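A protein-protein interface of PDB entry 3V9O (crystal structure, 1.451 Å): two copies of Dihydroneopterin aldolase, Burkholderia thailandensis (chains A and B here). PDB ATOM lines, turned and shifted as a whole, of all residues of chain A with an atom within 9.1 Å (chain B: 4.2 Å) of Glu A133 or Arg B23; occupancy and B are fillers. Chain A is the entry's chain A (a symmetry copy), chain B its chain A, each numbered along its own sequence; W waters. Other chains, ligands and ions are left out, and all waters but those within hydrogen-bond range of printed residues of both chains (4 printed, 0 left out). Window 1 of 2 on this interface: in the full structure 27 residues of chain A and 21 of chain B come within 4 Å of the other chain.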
ATOM      1  N   ASN A  52     -23.847 -19.213  29.999  1.00  0.00           N
ATOM      2  CA  ASN A  52     -24.583 -20.419  29.636  1.00  0.00           C
ATOM      3  C   ASN A  52     -23.607 -21.409  29.084  1.00  0.00           C
ATOM      4  O   ASN A  52     -22.671 -21.057  28.359  1.00  0.00           O
ATOM      5  CB  ASN A  52     -25.660 -20.096  28.558  1.00  0.00           C
ATOM      6  CG  ASN A  52     -26.826 -19.405  29.169  1.00  0.00           C
ATOM      7  OD1 ASN A  52     -27.733 -20.068  29.632  1.00  0.00           O
ATOM      8  ND2 ASN A  52     -26.792 -18.064  29.268  1.00  0.00           N
ATOM      9  N   VAL A  53     -23.795 -22.693  29.442  1.00  0.00           N
ATOM     10  CA  VAL A  53     -22.832 -23.750  29.034  1.00  0.00           C
ATOM     11  C   VAL A  53     -23.628 -24.969  28.572  1.00  0.00           C
ATOM     12  O   VAL A  53     -24.631 -25.372  29.189  1.00  0.00           O
ATOM     13  CB  VAL A  53     -21.974 -24.209  30.222  1.00  0.00           C
ATOM     14  CG1 VAL A  53     -20.949 -25.313  29.806  1.00  0.00           C
ATOM     15  CG2 VAL A  53     -21.209 -22.984  30.838  1.00  0.00           C
ATOM     16  N   ASP A  54     -23.148 -25.559  27.471  1.00  0.00           N
ATOM     17  CA  ASP A  54     -23.667 -26.853  26.960  1.00  0.00           C
ATOM     18  C   ASP A  54     -22.438 -27.756  26.852  1.00  0.00           C
ATOM     19  O   ASP A  54     -21.412 -27.416  26.256  1.00  0.00           O
ATOM     20  CB  ASP A  54     -24.318 -26.761  25.595  1.00  0.00           C
ATOM     21  CG  ASP A  54     -25.567 -25.949  25.569  1.00  0.00           C
ATOM     22  OD1 ASP A  54     -26.507 -26.210  26.307  1.00  0.00           O
ATOM     23  OD2 ASP A  54     -25.636 -25.053  24.713  1.00  0.00           O
ATOM     24  N   LEU A  93     -11.716  -8.637  28.841  1.00  0.00           N
ATOM     25  CA  LEU A  93     -12.611  -8.941  27.725  1.00  0.00           C
ATOM     26  C   LEU A  93     -13.494 -10.133  27.993  1.00  0.00           C
ATOM     27  O   LEU A  93     -13.075 -11.129  28.621  1.00  0.00           O
ATOM     28  CB  LEU A  93     -11.757  -9.274  26.481  1.00  0.00           C
ATOM     29  CG  LEU A  93     -10.804  -8.227  25.993  1.00  0.00           C
ATOM     30  CD1 LEU A  93     -10.010  -8.780  24.811  1.00  0.00           C
ATOM     31  CD2 LEU A  93     -11.629  -7.046  25.595  1.00  0.00           C
ATOM     32  N   GLN A  94     -14.717 -10.114  27.459  1.00  0.00           N
ATOM     33  CA  GLN A  94     -15.590 -11.283  27.510  1.00  0.00           C
ATOM     34  C   GLN A  94     -14.932 -12.471  26.813  1.00  0.00           C
ATOM     35  O   GLN A  94     -15.062 -13.590  27.314  1.00  0.00           O
ATOM     36  CB  GLN A  94     -16.947 -11.002  26.854  1.00  0.00           C
ATOM     37  CG  GLN A  94     -17.801 -10.011  27.666  1.00  0.00           C
ATOM     38  CD  GLN A  94     -19.278 -10.162  27.340  1.00  0.00           C
ATOM     39  OE1 GLN A  94     -19.830 -11.251  27.342  1.00  0.00           O
ATOM     40  NE2 GLN A  94     -19.966  -9.046  27.052  1.00  0.00           N
ATOM     41  N   GLU A  95     -14.232 -12.270  25.702  1.00  0.00           N
ATOM     42  CA  GLU A  95     -13.554 -13.372  25.019  1.00  0.00           C
ATOM     43  C   GLU A  95     -12.588 -14.079  25.945  1.00  0.00           C
ATOM     44  O   GLU A  95     -12.506 -15.299  25.907  1.00  0.00           O
ATOM     45  CB  GLU A  95     -12.762 -12.883  23.813  1.00  0.00           C
ATOM     46  CG  GLU A  95     -13.630 -12.498  22.590  1.00  0.00           C
ATOM     47  CD  GLU A  95     -14.241 -11.093  22.644  1.00  0.00           C
ATOM     48  OE1 GLU A  95     -14.274 -10.404  23.692  1.00  0.00           O
ATOM     49  OE2 GLU A  95     -14.705 -10.654  21.579  1.00  0.00           O
ATOM     50  N   THR A  96     -11.879 -13.329  26.775  1.00  0.00           N
ATOM     51  CA  THR A  96     -10.912 -13.972  27.693  1.00  0.00           C
ATOM     52  C   THR A  96     -11.622 -14.946  28.631  1.00  0.00           C
ATOM     53  O   THR A  96     -11.188 -16.086  28.791  1.00  0.00           O
ATOM     54  CB  THR A  96     -10.173 -12.926  28.437  1.00  0.00           C
ATOM     55  OG1 THR A  96      -9.423 -12.144  27.487  1.00  0.00           O
ATOM     56  CG2 THR A  96      -9.210 -13.523  29.440  1.00  0.00           C
ATOM     57  N   LEU A  97     -12.758 -14.557  29.184  1.00  0.00           N
ATOM     58  CA  LEU A  97     -13.491 -15.422  30.095  1.00  0.00           C
ATOM     59  C   LEU A  97     -14.136 -16.552  29.340  1.00  0.00           C
ATOM     60  O   LEU A  97     -14.038 -17.715  29.790  1.00  0.00           O
ATOM     61  CB  LEU A  97     -14.552 -14.561  30.801  1.00  0.00           C
ATOM     62  CG  LEU A  97     -15.456 -15.358  31.758  1.00  0.00           C
ATOM     63  CD1 LEU A  97     -14.703 -15.992  32.878  1.00  0.00           C
ATOM     64  CD2 LEU A  97     -16.605 -14.430  32.330  1.00  0.00           C
ATOM     65  N   CYS A  98     -14.805 -16.267  28.235  1.00  0.00           N
ATOM     66  CA  CYS A  98     -15.498 -17.290  27.500  1.00  0.00           C
ATOM     67  C   CYS A  98     -14.550 -18.379  27.003  1.00  0.00           C
ATOM     68  O   CYS A  98     -14.868 -19.570  27.143  1.00  0.00           O
ATOM     69  CB  CYS A  98     -16.219 -16.601  26.331  1.00  0.00           C
ATOM     70  SG  CYS A  98     -17.389 -17.669  25.459  1.00  0.00           S
ATOM     71  N   ASP A  99     -13.452 -17.965  26.423  1.00  0.00           N
ATOM     72  CA  ASP A  99     -12.483 -18.912  25.885  1.00  0.00           C
ATOM     73  C   ASP A  99     -11.879 -19.744  27.025  1.00  0.00           C
ATOM     74  O   ASP A  99     -11.623 -20.967  26.822  1.00  0.00           O
ATOM     75  CB  ASP A  99     -11.354 -18.169  25.187  1.00  0.00           C
ATOM     76  CG  ASP A  99     -11.770 -17.481  23.863  1.00  0.00           C
ATOM     77  OD1 ASP A  99     -12.918 -17.650  23.380  1.00  0.00           O
ATOM     78  OD2 ASP A  99     -10.897 -16.756  23.342  1.00  0.00           O
ATOM     79  N   ALA A 100     -11.633 -19.151  28.203  1.00  0.00           N
ATOM     80  CA  ALA A 100     -11.051 -19.890  29.306  1.00  0.00           C
ATOM     81  C   ALA A 100     -12.004 -20.941  29.835  1.00  0.00           C
ATOM     82  O   ALA A 100     -11.557 -22.065  30.135  1.00  0.00           O
ATOM     83  CB  ALA A 100     -10.620 -18.944  30.432  1.00  0.00           C
ATOM     84  N   ALA A 102     -14.400 -22.406  28.064  1.00  0.00           N
ATOM     85  CA  ALA A 102     -14.453 -23.470  27.063  1.00  0.00           C
ATOM     86  C   ALA A 102     -13.214 -24.361  27.110  1.00  0.00           C
ATOM     87  O   ALA A 102     -13.352 -25.606  27.031  1.00  0.00           O
ATOM     88  CB  ALA A 102     -14.632 -22.893  25.651  1.00  0.00           C
ATOM     89  N   VAL A 114     -18.118 -28.399  23.539  1.00  0.00           N
ATOM     90  CA  VAL A 114     -18.706 -27.472  24.496  1.00  0.00           C
ATOM     91  C   VAL A 114     -19.163 -26.205  23.790  1.00  0.00           C
ATOM     92  O   VAL A 114     -18.539 -25.745  22.812  1.00  0.00           O
ATOM     93  CB  VAL A 114     -17.732 -27.239  25.661  1.00  0.00           C
ATOM     94  CG1 VAL A 114     -16.475 -26.583  25.177  1.00  0.00           C
ATOM     95  CG2 VAL A 114     -18.419 -26.395  26.776  1.00  0.00           C
ATOM     96  N   ARG A 115     -20.287 -25.653  24.255  1.00  0.00           N
ATOM     97  CA  ARG A 115     -20.758 -24.343  23.804  1.00  0.00           C
ATOM     98  C   ARG A 115     -20.701 -23.488  25.084  1.00  0.00           C
ATOM     99  O   ARG A 115     -21.271 -23.916  26.125  1.00  0.00           O
ATOM    100  CB  ARG A 115     -22.174 -24.380  23.248  1.00  0.00           C
ATOM    101  CG  ARG A 115     -22.601 -22.965  22.687  1.00  0.00           C
ATOM    102  CD  ARG A 115     -24.052 -22.959  22.189  1.00  0.00           C
ATOM    103  NE  ARG A 115     -24.981 -23.088  23.339  1.00  0.00           N
ATOM    104  CZ  ARG A 115     -25.425 -22.087  24.145  1.00  0.00           C
ATOM    105  NH1 ARG A 115     -25.054 -20.806  24.003  1.00  0.00           N
ATOM    106  NH2 ARG A 115     -26.264 -22.389  25.144  1.00  0.00           N
ATOM    107  N   VAL A 116     -20.104 -22.310  25.047  1.00  0.00           N
ATOM    108  CA  VAL A 116     -20.088 -21.369  26.173  1.00  0.00           C
ATOM    109  C   VAL A 116     -20.434 -19.995  25.649  1.00  0.00           C
ATOM    110  O   VAL A 116     -19.941 -19.565  24.611  1.00  0.00           O
ATOM    111  CB  VAL A 116     -18.718 -21.246  26.801  1.00  0.00           C
ATOM    112  CG1 VAL A 116     -18.784 -20.280  28.026  1.00  0.00           C
ATOM    113  CG2 VAL A 116     -18.193 -22.617  27.215  1.00  0.00           C
ATOM    114  N   SER A 117     -21.365 -19.329  26.330  1.00  0.00           N
ATOM    115  CA  SER A 117     -21.622 -17.909  26.089  1.00  0.00           C
ATOM    116  C   SER A 117     -21.446 -17.155  27.400  1.00  0.00           C
ATOM    117  O   SER A 117     -21.813 -17.629  28.493  1.00  0.00           O
ATOM    118  CB  SER A 117     -22.998 -17.617  25.452  1.00  0.00           C
ATOM    119  OG  SER A 117     -24.048 -17.956  26.346  1.00  0.00           O
ATOM    120  N   THR A 118     -20.922 -15.954  27.270  1.00  0.00           N
ATOM    121  CA  THR A 118     -20.952 -14.947  28.344  1.00  0.00           C
ATOM    122  C   THR A 118     -21.703 -13.740  27.835  1.00  0.00           C
ATOM    123  O   THR A 118     -21.721 -13.483  26.629  1.00  0.00           O
ATOM    124  CB  THR A 118     -19.513 -14.514  28.802  1.00  0.00           C
ATOM    125  OG1 THR A 118     -18.845 -13.925  27.677  1.00  0.00           O
ATOM    126  CG2 THR A 118     -18.674 -15.770  29.247  1.00  0.00           C
ATOM    127  N   GLU A 119     -22.362 -13.006  28.747  1.00  0.00           N
ATOM    128  CA  GLU A 119     -23.012 -11.758  28.314  1.00  0.00           C
ATOM    129  C   GLU A 119     -23.071 -10.836  29.486  1.00  0.00           C
ATOM    130  O   GLU A 119     -23.084 -11.211  30.655  1.00  0.00           O
ATOM    131  CB  GLU A 119     -24.390 -12.059  27.704  1.00  0.00           C
ATOM    132  CG  GLU A 119     -25.409 -12.553  28.749  1.00  0.00           C
ATOM    133  CD  GLU A 119     -26.656 -13.151  28.166  1.00  0.00           C
ATOM    134  OE1 GLU A 119     -26.556 -13.848  27.147  1.00  0.00           O
ATOM    135  OE2 GLU A 119     -27.728 -13.040  28.812  1.00  0.00           O
ATOM    136  N   VAL A 130     -25.230  -7.846  25.730  1.00  0.00           N
ATOM    137  CA  VAL A 130     -24.291  -8.058  24.636  1.00  0.00           C
ATOM    138  C   VAL A 130     -23.374  -9.178  25.121  1.00  0.00           C
ATOM    139  O   VAL A 130     -22.948  -9.171  26.284  1.00  0.00           O
ATOM    140  CB  VAL A 130     -23.514  -6.733  24.294  1.00  0.00           C
ATOM    141  CG1 VAL A 130     -22.594  -6.298  25.426  1.00  0.00           C
ATOM    142  CG2 VAL A 130     -22.731  -6.875  22.973  1.00  0.00           C
ATOM    143  N   GLY A 131     -23.057 -10.076  24.210  1.00  0.00           N
ATOM    144  CA  GLY A 131     -22.308 -11.266  24.605  1.00  0.00           C
ATOM    145  C   GLY A 131     -21.483 -11.840  23.499  1.00  0.00           C
ATOM    146  O   GLY A 131     -21.409 -11.386  22.363  1.00  0.00           O
ATOM    147  N   VAL A 132     -20.763 -12.895  23.925  1.00  0.00           N
ATOM    148  CA  VAL A 132     -19.808 -13.650  23.109  1.00  0.00           C
ATOM    149  C   VAL A 132     -20.077 -15.138  23.268  1.00  0.00           C
ATOM    150  O   VAL A 132     -20.295 -15.597  24.414  1.00  0.00           O
ATOM    151  CB  VAL A 132     -18.346 -13.343  23.537  1.00  0.00           C
ATOM    152  CG1 VAL A 132     -17.321 -14.272  22.772  1.00  0.00           C
ATOM    153  CG2 VAL A 132     -18.086 -11.825  23.351  1.00  0.00           C
ATOM    154  N   GLU A 133     -20.023 -15.899  22.182  1.00  0.00           N
ATOM    155  CA  GLU A 133     -20.257 -17.357  22.270  1.00  0.00           C
ATOM    156  C   GLU A 133     -19.227 -18.075  21.437  1.00  0.00           C
ATOM    157  O   GLU A 133     -18.875 -17.646  20.320  1.00  0.00           O
ATOM    158  CB  GLU A 133     -21.653 -17.668  21.763  1.00  0.00           C
ATOM    159  CG  GLU A 133     -21.980 -19.201  21.761  1.00  0.00           C
ATOM    160  CD  GLU A 133     -23.312 -19.441  21.176  1.00  0.00           C
ATOM    161  OE1 GLU A 133     -23.400 -19.373  19.955  1.00  0.00           O
ATOM    162  OE2 GLU A 133     -24.287 -19.607  21.941  1.00  0.00           O
ATOM    163  N   VAL A 134     -18.760 -19.206  21.969  1.00  0.00           N
ATOM    164  CA  VAL A 134     -17.952 -20.144  21.199  1.00  0.00           C
ATOM    165  C   VAL A 134     -18.543 -21.534  21.232  1.00  0.00           C
ATOM    166  O   VAL A 134     -19.253 -21.884  22.198  1.00  0.00           O
ATOM    167  CB  VAL A 134     -16.503 -20.251  21.654  1.00  0.00           C
ATOM    168  CG1 VAL A 134     -15.832 -18.847  21.547  1.00  0.00           C
ATOM    169  CG2 VAL A 134     -16.369 -20.757  23.037  1.00  0.00           C
ATOM    170  N   PHE A 135     -18.262 -22.335  20.232  1.00  0.00           N
ATOM    171  CA  PHE A 135     -18.711 -23.743  20.157  1.00  0.00           C
ATOM    172  C   PHE A 135     -17.550 -24.523  19.583  1.00  0.00           C
ATOM    173  O   PHE A 135     -17.172 -24.318  18.425  1.00  0.00           O
ATOM    174  CB  PHE A 135     -19.963 -23.845  19.255  1.00  0.00           C
ATOM    175  CG  PHE A 135     -20.882 -25.046  19.516  1.00  0.00           C
ATOM    176  CD1 PHE A 135     -20.410 -26.243  19.993  1.00  0.00           C
ATOM    177  CD2 PHE A 135     -22.259 -24.930  19.284  1.00  0.00           C
ATOM    178  CE1 PHE A 135     -21.275 -27.378  20.133  1.00  0.00           C
ATOM    179  CE2 PHE A 135     -23.146 -26.021  19.493  1.00  0.00           C
ATOM    180  CZ  PHE A 135     -22.632 -27.243  19.929  1.00  0.00           C
ATOM    181  N   ARG A 136     -16.963 -25.340  20.413  1.00  0.00           N
ATOM    182  CA  ARG A 136     -15.760 -26.096  20.081  1.00  0.00           C
ATOM    183  C   ARG A 136     -16.057 -27.589  20.096  1.00  0.00           C
ATOM    184  O   ARG A 136     -16.578 -28.108  21.078  1.00  0.00           O
ATOM    185  CB  ARG A 136     -14.667 -25.792  21.112  1.00  0.00           C
ATOM    186  CG  ARG A 136     -14.094 -24.346  21.100  1.00  0.00           C
ATOM    187  CD  ARG A 136     -13.314 -24.025  19.814  1.00  0.00           C
ATOM    188  NE  ARG A 136     -14.251 -23.624  18.778  1.00  0.00           N
ATOM    189  CZ  ARG A 136     -14.077 -23.760  17.466  1.00  0.00           C
ATOM    190  NH1 ARG A 136     -12.967 -24.294  16.965  1.00  0.00           N
ATOM    191  NH2 ARG A 136     -15.040 -23.359  16.657  1.00  0.00           N
ATOM    192  N   LEU B  14     -23.009 -21.966  14.983  1.00  0.00           N
ATOM    193  CA  LEU B  14     -21.555 -22.168  14.978  1.00  0.00           C
ATOM    194  C   LEU B  14     -21.164 -23.607  14.569  1.00  0.00           C
ATOM    195  O   LEU B  14     -19.980 -23.959  14.536  1.00  0.00           O
ATOM    196  CB  LEU B  14     -20.911 -21.741  16.315  1.00  0.00           C
ATOM    197  CG  LEU B  14     -20.913 -20.241  16.677  1.00  0.00           C
ATOM    198  CD1 LEU B  14     -20.452 -20.023  18.106  1.00  0.00           C
ATOM    199  CD2 LEU B  14     -20.042 -19.437  15.766  1.00  0.00           C
ATOM    200  N   CYS B  22     -15.421 -19.626  13.694  1.00  0.00           N
ATOM    201  CA  CYS B  22     -15.837 -18.300  14.140  1.00  0.00           C
ATOM    202  C   CYS B  22     -16.326 -18.318  15.609  1.00  0.00           C
ATOM    203  O   CYS B  22     -16.736 -19.358  16.133  1.00  0.00           O
ATOM    204  CB  CYS B  22     -17.013 -17.762  13.314  1.00  0.00           C
ATOM    205  SG  CYS B  22     -16.444 -17.260  11.667  1.00  0.00           S
ATOM    206  N   ARG B  23     -16.217 -17.189  16.252  1.00  0.00           N
ATOM    207  CA  ARG B  23     -17.044 -16.912  17.444  1.00  0.00           C
ATOM    208  C   ARG B  23     -18.223 -16.054  17.047  1.00  0.00           C
ATOM    209  O   ARG B  23     -18.246 -15.439  15.961  1.00  0.00           O
ATOM    210  CB  ARG B  23     -16.225 -16.224  18.548  1.00  0.00           C
ATOM    211  CG  ARG B  23     -15.829 -14.799  18.234  1.00  0.00           C
ATOM    212  CD  ARG B  23     -15.116 -14.136  19.463  1.00  0.00           C
ATOM    213  NE  ARG B  23     -13.739 -14.642  19.715  1.00  0.00           N
ATOM    214  CZ  ARG B  23     -13.369 -15.415  20.740  1.00  0.00           C
ATOM    215  NH1 ARG B  23     -14.201 -15.886  21.614  1.00  0.00           N
ATOM    216  NH2 ARG B  23     -12.080 -15.687  20.914  1.00  0.00           N
ATOM    217  N   ARG B  24     -19.228 -16.048  17.895  1.00  0.00           N
ATOM    218  CA  ARG B  24     -20.445 -15.242  17.676  1.00  0.00           C
ATOM    219  C   ARG B  24     -20.489 -14.123  18.678  1.00  0.00           C
ATOM    220  O   ARG B  24     -20.416 -14.354  19.889  1.00  0.00           O
ATOM    221  CB  ARG B  24     -21.677 -16.114  17.849  1.00  0.00           C
ATOM    222  CG  ARG B  24     -23.015 -15.340  17.764  1.00  0.00           C
ATOM    223  CD  ARG B  24     -24.209 -16.322  17.673  1.00  0.00           C
ATOM    224  NE  ARG B  24     -24.476 -16.986  18.950  1.00  0.00           N
ATOM    225  CZ  ARG B  24     -25.411 -16.591  19.833  1.00  0.00           C
ATOM    226  NH1 ARG B  24     -26.174 -15.534  19.582  1.00  0.00           N
ATOM    227  NH2 ARG B  24     -25.592 -17.273  20.976  1.00  0.00           N
ATOM    228  N   LEU B  25     -20.576 -12.883  18.227  1.00  0.00           N
ATOM    229  CA  LEU B  25     -20.853 -11.732  19.079  1.00  0.00           C
ATOM    230  C   LEU B  25     -22.333 -11.447  18.908  1.00  0.00           C
ATOM    231  O   LEU B  25     -22.851 -11.603  17.810  1.00  0.00           O
ATOM    232  CB  LEU B  25     -20.060 -10.527  18.569  1.00  0.00           C
ATOM    233  CG  LEU B  25     -18.545 -10.738  18.296  1.00  0.00           C
ATOM    234  CD1 LEU B  25     -17.963  -9.429  17.785  1.00  0.00           C
ATOM    235  CD2 LEU B  25     -17.799 -11.180  19.527  1.00  0.00           C
ATOM    236  N   LEU B  55     -23.025 -11.337  15.031  1.00  0.00           N
ATOM    237  CA  LEU B  55     -21.902 -11.113  14.150  1.00  0.00           C
ATOM    238  C   LEU B  55     -20.957 -12.306  14.273  1.00  0.00           C
ATOM    239  O   LEU B  55     -20.554 -12.664  15.402  1.00  0.00           O
ATOM    240  CB  LEU B  55     -21.259  -9.781  14.610  1.00  0.00           C
ATOM    241  CG  LEU B  55     -20.435  -8.963  13.691  1.00  0.00           C
ATOM    242  CD1 LEU B  55     -21.342  -8.549  12.509  1.00  0.00           C
ATOM    243  CD2 LEU B  55     -20.018  -7.712  14.475  1.00  0.00           C
ATOM    244  N   PHE B  56     -20.577 -12.941  13.172  1.00  0.00           N
ATOM    245  CA  PHE B  56     -19.639 -14.101  13.173  1.00  0.00           C
ATOM    246  C   PHE B  56     -18.290 -13.619  12.742  1.00  0.00           C
ATOM    247  O   PHE B  56     -18.164 -13.113  11.607  1.00  0.00           O
ATOM    248  CB  PHE B  56     -20.177 -15.259  12.337  1.00  0.00           C
ATOM    249  CG  PHE B  56     -21.520 -15.737  12.882  1.00  0.00           C
ATOM    250  CD1 PHE B  56     -22.731 -15.131  12.509  1.00  0.00           C
ATOM    251  CD2 PHE B  56     -21.494 -16.789  13.793  1.00  0.00           C
ATOM    252  CE1 PHE B  56     -23.957 -15.566  13.099  1.00  0.00           C
ATOM    253  CE2 PHE B  56     -22.691 -17.239  14.334  1.00  0.00           C
ATOM    254  CZ  PHE B  56     -23.891 -16.642  13.973  1.00  0.00           C
ATOM    255  N   VAL B  57     -17.314 -13.720  13.639  1.00  0.00           N
ATOM    256  CA  VAL B  57     -15.956 -13.243  13.377  1.00  0.00           C
ATOM    257  C   VAL B  57     -14.956 -14.406  13.570  1.00  0.00           C
ATOM    258  O   VAL B  57     -15.109 -15.188  14.543  1.00  0.00           O
ATOM    259  CB  VAL B  57     -15.639 -12.004  14.281  1.00  0.00           C
ATOM    260  CG1 VAL B  57     -16.655 -10.910  14.021  1.00  0.00           C
ATOM    261  CG2 VAL B  57     -15.699 -12.356  15.768  1.00  0.00           C
ATOM    262  N   LEU B  59     -12.203 -16.890  14.827  1.00  0.00           N
ATOM    263  CA  LEU B  59     -11.326 -17.051  15.984  1.00  0.00           C
ATOM    264  C   LEU B  59      -9.920 -16.597  15.691  1.00  0.00           C
ATOM    265  O   LEU B  59      -9.256 -16.015  16.542  1.00  0.00           O
ATOM    266  CB  LEU B  59     -11.332 -18.519  16.445  1.00  0.00           C
ATOM    267  CG  LEU B  59     -12.721 -19.000  16.923  1.00  0.00           C
ATOM    268  CD1 LEU B  59     -12.769 -20.511  17.166  1.00  0.00           C
ATOM    269  CD2 LEU B  59     -13.143 -18.264  18.205  1.00  0.00           C
ATOM    270  N   THR B  62      -9.609 -13.037  16.401  1.00  0.00           N
ATOM    271  CA  THR B  62     -10.272 -12.462  17.600  1.00  0.00           C
ATOM    272  C   THR B  62      -9.994 -13.266  18.836  1.00  0.00           C
ATOM    273  O   THR B  62     -10.831 -13.345  19.737  1.00  0.00           O
ATOM    274  CB  THR B  62     -11.805 -12.340  17.443  1.00  0.00           C
ATOM    275  OG1 THR B  62     -12.379 -13.646  17.279  1.00  0.00           O
ATOM    276  CG2 THR B  62     -12.155 -11.446  16.254  1.00  0.00           C
ATOM    277  N   THR B  63      -8.818 -13.883  18.920  1.00  0.00           N
ATOM    278  CA  THR B  63      -8.459 -14.694  20.085  1.00  0.00           C
ATOM    279  C   THR B  63      -7.433 -13.927  20.850  1.00  0.00           C
ATOM    280  O   THR B  63      -6.286 -13.855  20.422  1.00  0.00           O
ATOM    281  CB  THR B  63      -7.975 -16.140  19.687  1.00  0.00           C
ATOM    282  OG1 THR B  63      -9.094 -16.836  19.079  1.00  0.00           O
ATOM    283  CG2 THR B  63      -7.550 -16.919  20.962  1.00  0.00           C
ATOM    284  N   PRO B  64      -7.834 -13.287  21.963  1.00  0.00           N
ATOM    285  CA  PRO B  64      -6.882 -12.496  22.728  1.00  0.00           C
ATOM    286  C   PRO B  64      -5.963 -13.374  23.523  1.00  0.00           C
ATOM    287  O   PRO B  64      -6.386 -14.339  24.204  1.00  0.00           O
ATOM    288  CB  PRO B  64      -7.770 -11.663  23.665  1.00  0.00           C
ATOM    289  CG  PRO B  64      -8.980 -12.593  23.894  1.00  0.00           C
ATOM    290  CD  PRO B  64      -9.191 -13.272  22.546  1.00  0.00           C
HETATM  291  O   HOH W   1      -6.712 -12.953  26.869  1.00  0.00           O
HETATM  292  O   HOH W   2      -8.670 -16.168  24.775  1.00  0.00           O
HETATM  293  O   HOH W   3     -17.398 -25.342  15.397  1.00  0.00           O
HETATM  294  O   HOH W   4     -16.564 -21.230  18.136  1.00  0.00           O
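The side-chain carboxylate (OD1) of Asp A99 lies within salt-bridge range of the guanidinium group (NH1) of Arg B23 (2.8 Å).
OE1 of Glu A133 lies within salt-bridge range of NE of Arg B24 (2.8 Å).
The backbone NH (N) of Arg B23 sits at hydrogen-bond distance from the backbone carbonyl oxygen (O) of Val B57, at 2.9 Å.
O of Leu B25 lies within hydrogen-bond range of N of Leu B55 (2.8 Å).
O of Leu B59 lies within hydrogen-bond range of OG1 of Thr B63, 2.7 Å away.
The side-chain sulfur (SG) of Cys A98 sits at hydrogen-bond distance from the backbone carbonyl oxygen (O) of Val A132 (3.7 Å).
OE2 of Glu A133 lies within salt-bridge range of NH1 of Arg A115.
O of Val A116 lies within hydrogen-bond range of N of Val A134 (2.9 Å).
Leu A93 touches Pro B64 (CD1 to CB, 3.8 Å).
Leu B25 touches Glu A95 (CD2 to OE2, 3.7 Å).
Thr A96 touches Pro B64.
Asp A99 touches Pro B64 (OD2 to CD, 3.96 Å).
Arg B23 touches Val A132.
Val A132 touches Arg B24 (CA to O, 3.4 Å).
Leu B25 touches Val A132.
Arg B23 touches Glu A133.
Leu B14 touches Phe A135 (CB to CB, 3.7 Å).
Leu B59 touches Arg A136.
Printed residues of chain B within 4 Å of Glu A133: Leu B14 (3.5 Å), Arg B23 (3.5 Å) and Arg B24 (2.8 Å).
No residue of chain A comes within 4 Å of Cys B22.
Of the printed residues of chain B, Thr A96 touches Pro B64 (3.6 Å).
Of the printed residues of chain B, Val A134 touches Leu B14 and Arg B23.
Printed residues of chain B within 4 Å of Gly A131: Arg B24 and Leu B25.
Of the printed residues of chain B, Glu A95 touches Arg B23, Leu B25 and Pro B64.
Printed residues of chain A within 4 Å of Leu B14: Glu A133, Val A134 and Phe A135.
The nearest residue of chain A that does not touch Arg B23 is Cys A98 (5.2 Å).
The nearest printed residue of chain B that does not touch Asp A99 is Thr B63 (4.1 Å).
Hydrophobic or aromatic side chains of chain A that line the printed part of chain B: Leu A93, Val A132, Val A134 and Phe A135.
Among the printed residues, 19 pairs touch across the chains.
Among the printed residues, Asp or Glu carboxylates within 4 Å of a Lys or Arg side-chain nitrogen of the other chain: Asp A99 with Arg B23 (2.8 Å) and Glu A133 with Arg B24 (2.8 Å).
No position is printed for both chains.
Of the 19 pairs that touch across the chains among the printed residues, none has its exchanged pair printed and touching as well.
Water W2 bridges the side-chain carboxylate (OD2) of Asp A99 (2.7 Å) and the backbone carbonyl oxygen (O) of Pro B64 (3.0 Å).
Water W4 lies within hydrogen-bond range of O of Cys B22, N of Phe A135 and NH2 of Arg A136.
Water W1 bridges OG1 of Thr A96 (2.9 Å) and O of Pro B64 (3.0 Å).
Water W3 lies within hydrogen-bond range of O of Leu B14 (3.1 Å), O of Phe A135 (3.2 Å) and NH2 of Arg A136 (3.3 Å).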
